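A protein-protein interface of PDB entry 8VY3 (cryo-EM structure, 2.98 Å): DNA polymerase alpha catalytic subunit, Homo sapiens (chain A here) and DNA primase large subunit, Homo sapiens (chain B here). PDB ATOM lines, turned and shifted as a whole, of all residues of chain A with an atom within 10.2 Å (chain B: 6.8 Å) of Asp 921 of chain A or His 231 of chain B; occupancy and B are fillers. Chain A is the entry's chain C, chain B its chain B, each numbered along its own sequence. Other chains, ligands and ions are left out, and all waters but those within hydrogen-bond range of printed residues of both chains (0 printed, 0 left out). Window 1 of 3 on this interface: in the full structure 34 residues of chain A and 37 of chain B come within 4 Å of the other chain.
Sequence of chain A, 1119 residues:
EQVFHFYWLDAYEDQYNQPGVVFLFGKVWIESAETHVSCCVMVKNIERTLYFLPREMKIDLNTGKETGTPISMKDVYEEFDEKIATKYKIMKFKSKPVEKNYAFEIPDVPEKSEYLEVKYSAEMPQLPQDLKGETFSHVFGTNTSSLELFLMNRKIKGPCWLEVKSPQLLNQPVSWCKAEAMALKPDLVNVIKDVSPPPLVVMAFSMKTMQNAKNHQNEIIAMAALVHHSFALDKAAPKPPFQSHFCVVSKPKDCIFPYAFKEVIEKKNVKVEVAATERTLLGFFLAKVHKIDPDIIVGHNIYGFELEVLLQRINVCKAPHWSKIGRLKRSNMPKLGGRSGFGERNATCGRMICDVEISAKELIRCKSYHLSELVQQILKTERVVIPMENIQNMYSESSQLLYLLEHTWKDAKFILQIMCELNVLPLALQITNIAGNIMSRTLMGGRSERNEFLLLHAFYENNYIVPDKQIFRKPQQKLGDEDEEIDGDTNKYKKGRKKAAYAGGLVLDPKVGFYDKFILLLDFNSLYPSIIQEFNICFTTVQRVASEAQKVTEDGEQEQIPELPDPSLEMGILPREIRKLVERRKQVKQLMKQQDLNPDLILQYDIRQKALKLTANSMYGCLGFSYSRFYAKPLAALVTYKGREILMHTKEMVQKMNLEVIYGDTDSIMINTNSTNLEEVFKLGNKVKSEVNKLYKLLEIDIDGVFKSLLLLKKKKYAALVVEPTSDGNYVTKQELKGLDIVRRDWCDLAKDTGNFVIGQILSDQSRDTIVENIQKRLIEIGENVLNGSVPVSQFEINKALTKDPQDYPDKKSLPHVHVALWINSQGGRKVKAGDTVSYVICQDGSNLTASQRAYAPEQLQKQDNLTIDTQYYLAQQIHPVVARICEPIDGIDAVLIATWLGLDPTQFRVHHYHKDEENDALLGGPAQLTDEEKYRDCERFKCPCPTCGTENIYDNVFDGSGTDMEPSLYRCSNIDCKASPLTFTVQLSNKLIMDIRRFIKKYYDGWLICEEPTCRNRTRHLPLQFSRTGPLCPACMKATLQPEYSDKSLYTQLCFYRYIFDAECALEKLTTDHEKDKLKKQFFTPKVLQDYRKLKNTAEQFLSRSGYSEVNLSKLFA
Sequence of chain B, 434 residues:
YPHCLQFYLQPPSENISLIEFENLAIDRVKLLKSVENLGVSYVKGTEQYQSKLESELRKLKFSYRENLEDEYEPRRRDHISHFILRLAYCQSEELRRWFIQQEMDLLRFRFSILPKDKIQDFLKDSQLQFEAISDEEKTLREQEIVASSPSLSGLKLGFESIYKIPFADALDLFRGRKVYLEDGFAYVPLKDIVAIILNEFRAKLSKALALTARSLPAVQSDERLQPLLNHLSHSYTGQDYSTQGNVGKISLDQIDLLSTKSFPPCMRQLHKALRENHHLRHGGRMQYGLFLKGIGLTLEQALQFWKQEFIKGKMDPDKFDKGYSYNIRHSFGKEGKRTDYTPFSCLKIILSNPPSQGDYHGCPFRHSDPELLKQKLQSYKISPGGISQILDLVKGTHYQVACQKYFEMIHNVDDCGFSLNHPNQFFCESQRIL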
ATOM      1  N   LEU A 508     -29.007 -23.665  17.908  1.00  0.00           N
ATOM      2  CA  LEU A 508     -27.783 -24.408  17.651  1.00  0.00           C
ATOM      3  C   LEU A 508     -28.073 -25.901  17.720  1.00  0.00           C
ATOM      4  O   LEU A 508     -28.662 -26.380  18.694  1.00  0.00           O
ATOM      5  CB  LEU A 508     -26.693 -24.029  18.653  1.00  0.00           C
ATOM      6  CG  LEU A 508     -26.351 -22.541  18.751  1.00  0.00           C
ATOM      7  CD1 LEU A 508     -25.387 -22.277  19.895  1.00  0.00           C
ATOM      8  CD2 LEU A 508     -25.772 -22.040  17.440  1.00  0.00           C
ATOM      9  N   ASP A 509     -27.668 -26.627  16.686  1.00  0.00           N
ATOM     10  CA  ASP A 509     -27.923 -28.059  16.614  1.00  0.00           C
ATOM     11  C   ASP A 509     -27.213 -28.776  17.755  1.00  0.00           C
ATOM     12  O   ASP A 509     -26.013 -28.543  17.970  1.00  0.00           O
ATOM     13  CB  ASP A 509     -27.457 -28.617  15.273  1.00  0.00           C
ATOM     14  CG  ASP A 509     -28.320 -28.156  14.118  1.00  0.00           C
ATOM     15  OD1 ASP A 509     -29.202 -27.299  14.338  1.00  0.00           O
ATOM     16  OD2 ASP A 509     -28.118 -28.651  12.990  1.00  0.00           O
ATOM     17  N   PRO A 510     -27.898 -29.634  18.509  1.00  0.00           N
ATOM     18  CA  PRO A 510     -27.240 -30.335  19.620  1.00  0.00           C
ATOM     19  C   PRO A 510     -26.130 -31.249  19.126  1.00  0.00           C
ATOM     20  O   PRO A 510     -26.207 -31.820  18.037  1.00  0.00           O
ATOM     21  CB  PRO A 510     -28.387 -31.124  20.261  1.00  0.00           C
ATOM     22  CG  PRO A 510     -29.383 -31.285  19.167  1.00  0.00           C
ATOM     23  CD  PRO A 510     -29.320 -29.997  18.403  1.00  0.00           C
ATOM     24  N   LYS A 511     -25.084 -31.376  19.939  1.00  0.00           N
ATOM     25  CA  LYS A 511     -24.007 -32.314  19.661  1.00  0.00           C
ATOM     26  C   LYS A 511     -24.352 -33.677  20.244  1.00  0.00           C
ATOM     27  O   LYS A 511     -24.005 -33.974  21.391  1.00  0.00           O
ATOM     28  CB  LYS A 511     -22.684 -31.802  20.231  1.00  0.00           C
ATOM     29  CG  LYS A 511     -21.570 -31.683  19.212  1.00  0.00           C
ATOM     30  CD  LYS A 511     -20.549 -30.643  19.634  1.00  0.00           C
ATOM     31  CE  LYS A 511     -20.668 -29.382  18.798  1.00  0.00           C
ATOM     32  NZ  LYS A 511     -19.510 -28.471  19.003  1.00  0.00           N
ATOM     33  N   VAL A 512     -25.033 -34.507  19.458  1.00  0.00           N
ATOM     34  CA  VAL A 512     -25.567 -35.788  19.908  1.00  0.00           C
ATOM     35  C   VAL A 512     -24.438 -36.703  20.367  1.00  0.00           C
ATOM     36  O   VAL A 512     -23.441 -36.877  19.659  1.00  0.00           O
ATOM     37  CB  VAL A 512     -26.389 -36.444  18.784  1.00  0.00           C
ATOM     38  CG1 VAL A 512     -26.737 -37.871  19.131  1.00  0.00           C
ATOM     39  CG2 VAL A 512     -27.641 -35.640  18.507  1.00  0.00           C
ATOM     40  N   MET A 648     -24.395 -16.136  19.062  1.00  0.00           N
ATOM     41  CA  MET A 648     -23.197 -16.578  18.353  1.00  0.00           C
ATOM     42  C   MET A 648     -21.940 -16.005  18.995  1.00  0.00           C
ATOM     43  O   MET A 648     -20.867 -16.615  18.946  1.00  0.00           O
ATOM     44  CB  MET A 648     -23.285 -16.183  16.879  1.00  0.00           C
ATOM     45  CG  MET A 648     -23.982 -17.214  16.010  1.00  0.00           C
ATOM     46  SD  MET A 648     -24.131 -16.693  14.293  1.00  0.00           S
ATOM     47  CE  MET A 648     -22.994 -17.826  13.499  1.00  0.00           C
ATOM     48  N   LYS A 651     -21.141 -18.210  22.048  1.00  0.00           N
ATOM     49  CA  LYS A 651     -20.581 -19.489  21.627  1.00  0.00           C
ATOM     50  C   LYS A 651     -19.100 -19.358  21.285  1.00  0.00           C
ATOM     51  O   LYS A 651     -18.304 -20.257  21.573  1.00  0.00           O
ATOM     52  CB  LYS A 651     -21.374 -20.032  20.438  1.00  0.00           C
ATOM     53  CG  LYS A 651     -21.121 -21.491  20.119  1.00  0.00           C
ATOM     54  CD  LYS A 651     -21.092 -21.723  18.620  1.00  0.00           C
ATOM     55  CE  LYS A 651     -20.075 -20.827  17.939  1.00  0.00           C
ATOM     56  NZ  LYS A 651     -20.059 -21.033  16.466  1.00  0.00           N
ATOM     57  N   LYS A 916     -29.084 -40.820   5.109  1.00  0.00           N
ATOM     58  CA  LYS A 916     -29.062 -39.471   5.665  1.00  0.00           C
ATOM     59  C   LYS A 916     -28.562 -39.481   7.106  1.00  0.00           C
ATOM     60  O   LYS A 916     -28.066 -38.469   7.615  1.00  0.00           O
ATOM     61  CB  LYS A 916     -30.462 -38.856   5.564  1.00  0.00           C
ATOM     62  CG  LYS A 916     -30.637 -37.512   6.248  1.00  0.00           C
ATOM     63  CD  LYS A 916     -31.950 -37.459   7.012  1.00  0.00           C
ATOM     64  CE  LYS A 916     -31.943 -36.354   8.055  1.00  0.00           C
ATOM     65  NZ  LYS A 916     -30.834 -36.520   9.032  1.00  0.00           N
ATOM     66  N   ASP A 917     -28.669 -40.629   7.775  1.00  0.00           N
ATOM     67  CA  ASP A 917     -28.269 -40.754   9.173  1.00  0.00           C
ATOM     68  C   ASP A 917     -26.782 -40.466   9.357  1.00  0.00           C
ATOM     69  O   ASP A 917     -26.351 -40.083  10.450  1.00  0.00           O
ATOM     70  CB  ASP A 917     -28.607 -42.152   9.700  1.00  0.00           C
ATOM     71  CG  ASP A 917     -28.623 -42.215  11.218  1.00  0.00           C
ATOM     72  OD1 ASP A 917     -28.569 -41.147  11.862  1.00  0.00           O
ATOM     73  OD2 ASP A 917     -28.692 -43.335  11.766  1.00  0.00           O
ATOM     74  N   GLU A 918     -25.990 -40.648   8.299  1.00  0.00           N
ATOM     75  CA  GLU A 918     -24.559 -40.375   8.376  1.00  0.00           C
ATOM     76  C   GLU A 918     -24.230 -38.892   8.278  1.00  0.00           C
ATOM     77  O   GLU A 918     -23.061 -38.526   8.440  1.00  0.00           O
ATOM     78  CB  GLU A 918     -23.814 -41.132   7.273  1.00  0.00           C
ATOM     79  CG  GLU A 918     -23.609 -42.608   7.557  1.00  0.00           C
ATOM     80  CD  GLU A 918     -22.969 -43.338   6.393  1.00  0.00           C
ATOM     81  OE1 GLU A 918     -23.003 -42.807   5.264  1.00  0.00           O
ATOM     82  OE2 GLU A 918     -22.430 -44.445   6.607  1.00  0.00           O
ATOM     83  N   GLU A 919     -25.218 -38.035   8.024  1.00  0.00           N
ATOM     84  CA  GLU A 919     -24.965 -36.604   7.897  1.00  0.00           C
ATOM     85  C   GLU A 919     -24.779 -35.966   9.269  1.00  0.00           C
ATOM     86  O   GLU A 919     -25.755 -35.582   9.921  1.00  0.00           O
ATOM     87  CB  GLU A 919     -26.105 -35.920   7.139  1.00  0.00           C
ATOM     88  CG  GLU A 919     -25.918 -35.902   5.628  1.00  0.00           C
ATOM     89  CD  GLU A 919     -27.041 -35.183   4.904  1.00  0.00           C
ATOM     90  OE1 GLU A 919     -27.407 -34.066   5.328  1.00  0.00           O
ATOM     91  OE2 GLU A 919     -27.556 -35.735   3.909  1.00  0.00           O
ATOM     92  N   ASN A 920     -23.527 -35.849   9.709  1.00  0.00           N
ATOM     93  CA  ASN A 920     -23.196 -35.267  11.004  1.00  0.00           C
ATOM     94  C   ASN A 920     -22.866 -33.787  10.911  1.00  0.00           C
ATOM     95  O   ASN A 920     -23.235 -33.018  11.806  1.00  0.00           O
ATOM     96  CB  ASN A 920     -22.020 -36.029  11.635  1.00  0.00           C
ATOM     97  CG  ASN A 920     -21.775 -35.635  13.078  1.00  0.00           C
ATOM     98  OD1 ASN A 920     -20.721 -35.931  13.642  1.00  0.00           O
ATOM     99  ND2 ASN A 920     -22.752 -34.971  13.687  1.00  0.00           N
ATOM    100  N   ASP A 921     -22.178 -33.363   9.855  1.00  0.00           N
ATOM    101  CA  ASP A 921     -21.832 -31.956   9.686  1.00  0.00           C
ATOM    102  C   ASP A 921     -22.650 -31.330   8.562  1.00  0.00           C
ATOM    103  O   ASP A 921     -23.880 -31.399   8.562  1.00  0.00           O
ATOM    104  CB  ASP A 921     -20.336 -31.794   9.403  1.00  0.00           C
ATOM    105  CG  ASP A 921     -19.469 -32.596  10.352  1.00  0.00           C
ATOM    106  OD1 ASP A 921     -19.595 -33.839  10.370  1.00  0.00           O
ATOM    107  OD2 ASP A 921     -18.661 -31.984  11.079  1.00  0.00           O
ATOM    108  N   GLN A 929     -14.808 -31.941  -1.186  1.00  0.00           N
ATOM    109  CA  GLN A 929     -15.777 -32.803  -1.847  1.00  0.00           C
ATOM    110  C   GLN A 929     -15.384 -34.273  -1.771  1.00  0.00           C
ATOM    111  O   GLN A 929     -14.322 -34.621  -1.260  1.00  0.00           O
ATOM    112  CB  GLN A 929     -15.955 -32.384  -3.310  1.00  0.00           C
ATOM    113  CG  GLN A 929     -16.850 -31.152  -3.597  1.00  0.00           C
ATOM    114  CD  GLN A 929     -18.057 -30.949  -2.665  1.00  0.00           C
ATOM    115  OE1 GLN A 929     -18.464 -31.835  -1.913  1.00  0.00           O
ATOM    116  NE2 GLN A 929     -18.632 -29.755  -2.728  1.00  0.00           N
ATOM    117  N   LYS A1049     -31.774 -35.807  -3.742  1.00  0.00           N
ATOM    118  CA  LYS A1049     -30.329 -35.952  -3.852  1.00  0.00           C
ATOM    119  C   LYS A1049     -29.941 -37.347  -4.317  1.00  0.00           C
ATOM    120  O   LYS A1049     -28.942 -37.507  -5.025  1.00  0.00           O
ATOM    121  CB  LYS A1049     -29.673 -35.632  -2.513  1.00  0.00           C
ATOM    122  CG  LYS A1049     -28.211 -35.254  -2.606  1.00  0.00           C
ATOM    123  CD  LYS A1049     -27.479 -35.579  -1.322  1.00  0.00           C
ATOM    124  CE  LYS A1049     -25.994 -35.725  -1.564  1.00  0.00           C
ATOM    125  NZ  LYS A1049     -25.198 -34.998  -0.541  1.00  0.00           N
ATOM    126  N   GLN B  91     -21.942 -14.229   8.180  1.00  0.00           N
ATOM    127  CA  GLN B  91     -22.626 -14.523   9.436  1.00  0.00           C
ATOM    128  C   GLN B  91     -21.960 -13.921  10.670  1.00  0.00           C
ATOM    129  O   GLN B  91     -22.558 -13.078  11.347  1.00  0.00           O
ATOM    130  CB  GLN B  91     -22.762 -16.035   9.616  1.00  0.00           C
ATOM    131  CG  GLN B  91     -23.594 -16.704   8.538  1.00  0.00           C
ATOM    132  CD  GLN B  91     -22.900 -17.893   7.913  1.00  0.00           C
ATOM    133  OE1 GLN B  91     -21.778 -18.235   8.281  1.00  0.00           O
ATOM    134  NE2 GLN B  91     -23.565 -18.529   6.956  1.00  0.00           N
ATOM    135  N   GLN B 226     -26.685 -25.876   2.333  1.00  0.00           N
ATOM    136  CA  GLN B 226     -26.395 -25.905   3.763  1.00  0.00           C
ATOM    137  C   GLN B 226     -24.931 -26.236   4.055  1.00  0.00           C
ATOM    138  O   GLN B 226     -24.359 -25.668   4.992  1.00  0.00           O
ATOM    139  CB  GLN B 226     -27.317 -26.900   4.477  1.00  0.00           C
ATOM    140  CG  GLN B 226     -28.795 -26.487   4.707  1.00  0.00           C
ATOM    141  CD  GLN B 226     -29.042 -25.070   5.242  1.00  0.00           C
ATOM    142  OE1 GLN B 226     -28.191 -24.185   5.190  1.00  0.00           O
ATOM    143  NE2 GLN B 226     -30.246 -24.862   5.758  1.00  0.00           N
ATOM    144  N   PRO B 227     -24.289 -27.152   3.318  1.00  0.00           N
ATOM    145  CA  PRO B 227     -22.838 -27.343   3.499  1.00  0.00           C
ATOM    146  C   PRO B 227     -21.991 -26.115   3.185  1.00  0.00           C
ATOM    147  O   PRO B 227     -20.839 -26.063   3.630  1.00  0.00           O
ATOM    148  CB  PRO B 227     -22.505 -28.497   2.540  1.00  0.00           C
ATOM    149  CG  PRO B 227     -23.748 -28.751   1.744  1.00  0.00           C
ATOM    150  CD  PRO B 227     -24.875 -28.291   2.590  1.00  0.00           C
ATOM    151  N   LEU B 228     -22.496 -25.141   2.429  1.00  0.00           N
ATOM    152  CA  LEU B 228     -21.739 -23.927   2.138  1.00  0.00           C
ATOM    153  C   LEU B 228     -21.814 -22.918   3.278  1.00  0.00           C
ATOM    154  O   LEU B 228     -20.784 -22.446   3.762  1.00  0.00           O
ATOM    155  CB  LEU B 228     -22.234 -23.276   0.835  1.00  0.00           C
ATOM    156  CG  LEU B 228     -22.056 -21.756   0.717  1.00  0.00           C
ATOM    157  CD1 LEU B 228     -21.389 -21.387  -0.593  1.00  0.00           C
ATOM    158  CD2 LEU B 228     -23.384 -21.031   0.850  1.00  0.00           C
ATOM    159  N   LEU B 229     -23.026 -22.582   3.717  1.00  0.00           N
ATOM    160  CA  LEU B 229     -23.205 -21.488   4.664  1.00  0.00           C
ATOM    161  C   LEU B 229     -22.508 -21.777   5.987  1.00  0.00           C
ATOM    162  O   LEU B 229     -21.896 -20.891   6.592  1.00  0.00           O
ATOM    163  CB  LEU B 229     -24.697 -21.233   4.889  1.00  0.00           C
ATOM    164  CG  LEU B 229     -25.523 -20.653   3.740  1.00  0.00           C
ATOM    165  CD1 LEU B 229     -26.915 -21.260   3.722  1.00  0.00           C
ATOM    166  CD2 LEU B 229     -25.602 -19.145   3.854  1.00  0.00           C
ATOM    167  N   ASN B 230     -22.587 -23.023   6.449  1.00  0.00           N
ATOM    168  CA  ASN B 230     -22.189 -23.317   7.819  1.00  0.00           C
ATOM    169  C   ASN B 230     -20.764 -23.851   7.915  1.00  0.00           C
ATOM    170  O   ASN B 230     -20.054 -23.545   8.879  1.00  0.00           O
ATOM    171  CB  ASN B 230     -23.168 -24.316   8.434  1.00  0.00           C
ATOM    172  CG  ASN B 230     -24.609 -23.877   8.300  1.00  0.00           C
ATOM    173  OD1 ASN B 230     -24.931 -23.003   7.498  1.00  0.00           O
ATOM    174  ND2 ASN B 230     -25.489 -24.491   9.081  1.00  0.00           N
ATOM    175  N   HIS B 231     -20.323 -24.638   6.939  1.00  0.00           N
ATOM    176  CA  HIS B 231     -19.155 -25.481   7.153  1.00  0.00           C
ATOM    177  C   HIS B 231     -18.074 -25.315   6.093  1.00  0.00           C
ATOM    178  O   HIS B 231     -17.587 -26.312   5.550  1.00  0.00           O
ATOM    179  CB  HIS B 231     -19.592 -26.945   7.212  1.00  0.00           C
ATOM    180  CG  HIS B 231     -20.573 -27.235   8.304  1.00  0.00           C
ATOM    181  ND1 HIS B 231     -20.598 -26.530   9.487  1.00  0.00           N
ATOM    182  CD2 HIS B 231     -21.581 -28.134   8.380  1.00  0.00           C
ATOM    183  CE1 HIS B 231     -21.570 -26.993  10.252  1.00  0.00           C
ATOM    184  NE2 HIS B 231     -22.182 -27.966   9.603  1.00  0.00           N
ATOM    185  N   LEU B 232     -17.685 -24.081   5.782  1.00  0.00           N
ATOM    186  CA  LEU B 232     -16.607 -23.889   4.819  1.00  0.00           C
ATOM    187  C   LEU B 232     -15.250 -23.810   5.507  1.00  0.00           C
ATOM    188  O   LEU B 232     -14.227 -23.616   4.844  1.00  0.00           O
ATOM    189  CB  LEU B 232     -16.839 -22.630   3.979  1.00  0.00           C
ATOM    190  CG  LEU B 232     -17.462 -22.823   2.595  1.00  0.00           C
ATOM    191  CD1 LEU B 232     -17.349 -21.554   1.773  1.00  0.00           C
ATOM    192  CD2 LEU B 232     -16.802 -23.975   1.867  1.00  0.00           C
ATOM    193  N   SER B 233     -15.228 -23.917   6.835  1.00  0.00           N
ATOM    194  CA  SER B 233     -13.967 -24.027   7.558  1.00  0.00           C
ATOM    195  C   SER B 233     -14.044 -24.906   8.806  1.00  0.00           C
ATOM    196  O   SER B 233     -13.180 -24.800   9.681  1.00  0.00           O
ATOM    197  CB  SER B 233     -13.480 -22.624   7.923  1.00  0.00           C
ATOM    198  OG  SER B 233     -14.566 -21.811   8.337  1.00  0.00           O
ATOM    199  N   HIS B 234     -15.056 -25.767   8.917  1.00  0.00           N
ATOM    200  CA  HIS B 234     -15.371 -26.329  10.229  1.00  0.00           C
ATOM    201  C   HIS B 234     -14.527 -27.545  10.615  1.00  0.00           C
ATOM    202  O   HIS B 234     -13.734 -27.466  11.560  1.00  0.00           O
ATOM    203  CB  HIS B 234     -16.864 -26.674  10.290  1.00  0.00           C
ATOM    204  CG  HIS B 234     -17.244 -27.559  11.438  1.00  0.00           C
ATOM    205  ND1 HIS B 234     -17.492 -28.907  11.292  1.00  0.00           N
ATOM    206  CD2 HIS B 234     -17.421 -27.285  12.753  1.00  0.00           C
ATOM    207  CE1 HIS B 234     -17.805 -29.426  12.466  1.00  0.00           C
ATOM    208  NE2 HIS B 234     -17.769 -28.463  13.370  1.00  0.00           N
ATOM    209  N   SER B 235     -14.671 -28.672   9.913  1.00  0.00           N
ATOM    210  CA  SER B 235     -13.910 -29.871  10.261  1.00  0.00           C
ATOM    211  C   SER B 235     -13.401 -30.657   9.059  1.00  0.00           C
ATOM    212  O   SER B 235     -12.581 -31.564   9.232  1.00  0.00           O
ATOM    213  CB  SER B 235     -14.748 -30.791  11.151  1.00  0.00           C
ATOM    214  OG  SER B 235     -14.569 -30.452  12.514  1.00  0.00           O
ATOM    215  N   TYR B 236     -13.881 -30.363   7.855  1.00  0.00           N
ATOM    216  CA  TYR B 236     -13.362 -31.003   6.651  1.00  0.00           C
ATOM    217  C   TYR B 236     -12.318 -30.103   5.998  1.00  0.00           C
ATOM    218  O   TYR B 236     -12.538 -28.899   5.823  1.00  0.00           O
ATOM    219  CB  TYR B 236     -14.494 -31.337   5.684  1.00  0.00           C
ATOM    220  CG  TYR B 236     -14.241 -32.602   4.898  1.00  0.00           C
ATOM    221  CD1 TYR B 236     -13.803 -33.757   5.528  1.00  0.00           C
ATOM    222  CD2 TYR B 236     -14.434 -32.637   3.526  1.00  0.00           C
ATOM    223  CE1 TYR B 236     -13.564 -34.908   4.814  1.00  0.00           C
ATOM    224  CE2 TYR B 236     -14.201 -33.782   2.804  1.00  0.00           C
ATOM    225  CZ  TYR B 236     -13.766 -34.915   3.451  1.00  0.00           C
ATOM    226  OH  TYR B 236     -13.535 -36.063   2.728  1.00  0.00           O
ATOM    227  N   ARG B 338     -17.379 -41.140   8.113  1.00  0.00           N
ATOM    228  CA  ARG B 338     -17.269 -39.744   8.526  1.00  0.00           C
ATOM    229  C   ARG B 338     -16.598 -39.566   9.881  1.00  0.00           C
ATOM    230  O   ARG B 338     -16.252 -38.439  10.249  1.00  0.00           O
ATOM    231  CB  ARG B 338     -18.647 -39.069   8.564  1.00  0.00           C
ATOM    232  CG  ARG B 338     -19.431 -39.077   7.257  1.00  0.00           C
ATOM    233  CD  ARG B 338     -18.933 -38.004   6.294  1.00  0.00           C
ATOM    234  NE  ARG B 338     -19.222 -38.321   4.899  1.00  0.00           N
ATOM    235  CZ  ARG B 338     -20.438 -38.399   4.374  1.00  0.00           C
ATOM    236  NH1 ARG B 338     -21.520 -38.142   5.091  1.00  0.00           N
ATOM    237  NH2 ARG B 338     -20.571 -38.735   3.094  1.00  0.00           N
ATOM    238  N   THR B 339     -16.410 -40.641  10.642  1.00  0.00           N
ATOM    239  CA  THR B 339     -15.566 -40.535  11.826  1.00  0.00           C
ATOM    240  C   THR B 339     -14.788 -41.820  12.083  1.00  0.00           C
ATOM    241  O   THR B 339     -13.915 -41.858  12.956  1.00  0.00           O
ATOM    242  CB  THR B 339     -16.413 -40.176  13.052  1.00  0.00           C
ATOM    243  OG1 THR B 339     -17.452 -39.266  12.673  1.00  0.00           O
ATOM    244  CG2 THR B 339     -15.556 -39.512  14.123  1.00  0.00           C
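O of Glu 918 of chain A touches NH1 of Arg 338 of chain B, at 3.7 Å.
CD2 of His 231 of chain B touches C of Asp 921 of chain A, 3.4 Å away.
Of chain B, only His 231 (3.4 Å) and His 234 (3.0 Å) come within 4 Å of Asp 921 of chain A.
No residue of chain A comes within 4 Å of Asn 230 of chain B.
No residue of chain A comes within 4 Å of Ser 233 of chain B.
Of the printed residues of chain B, Glu 918 of chain A touches Arg 338 (3.7 Å).
Of the printed residues of chain A, Arg 338 of chain B touches Glu 918 (3.7 Å).
Printed residues of chain A within 4 Å of His 234 of chain B: Asp 921 (3.0 Å).
Asp 509 of chain A touches none of the printed residues of chain B.
The nearest residue of chain B that does not touch Asp 921 of chain A is Ser 235 of chain B (4.1 Å).
The nearest printed residue of chain A that does not touch Arg 338 of chain B is Glu 919 of chain A (4.7 Å).
A ring nitrogen (ND1) of His 234 of chain B lies close to the side-chain carboxylate (OD2) of Asp 921 of chain A, at 3.3 Å.
Among the printed residues, 3 pairs touch across the chains.
Among the printed residues, no Asp or Glu carboxylate lies within 4 Å of a Lys or Arg side-chain nitrogen of the other chain.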
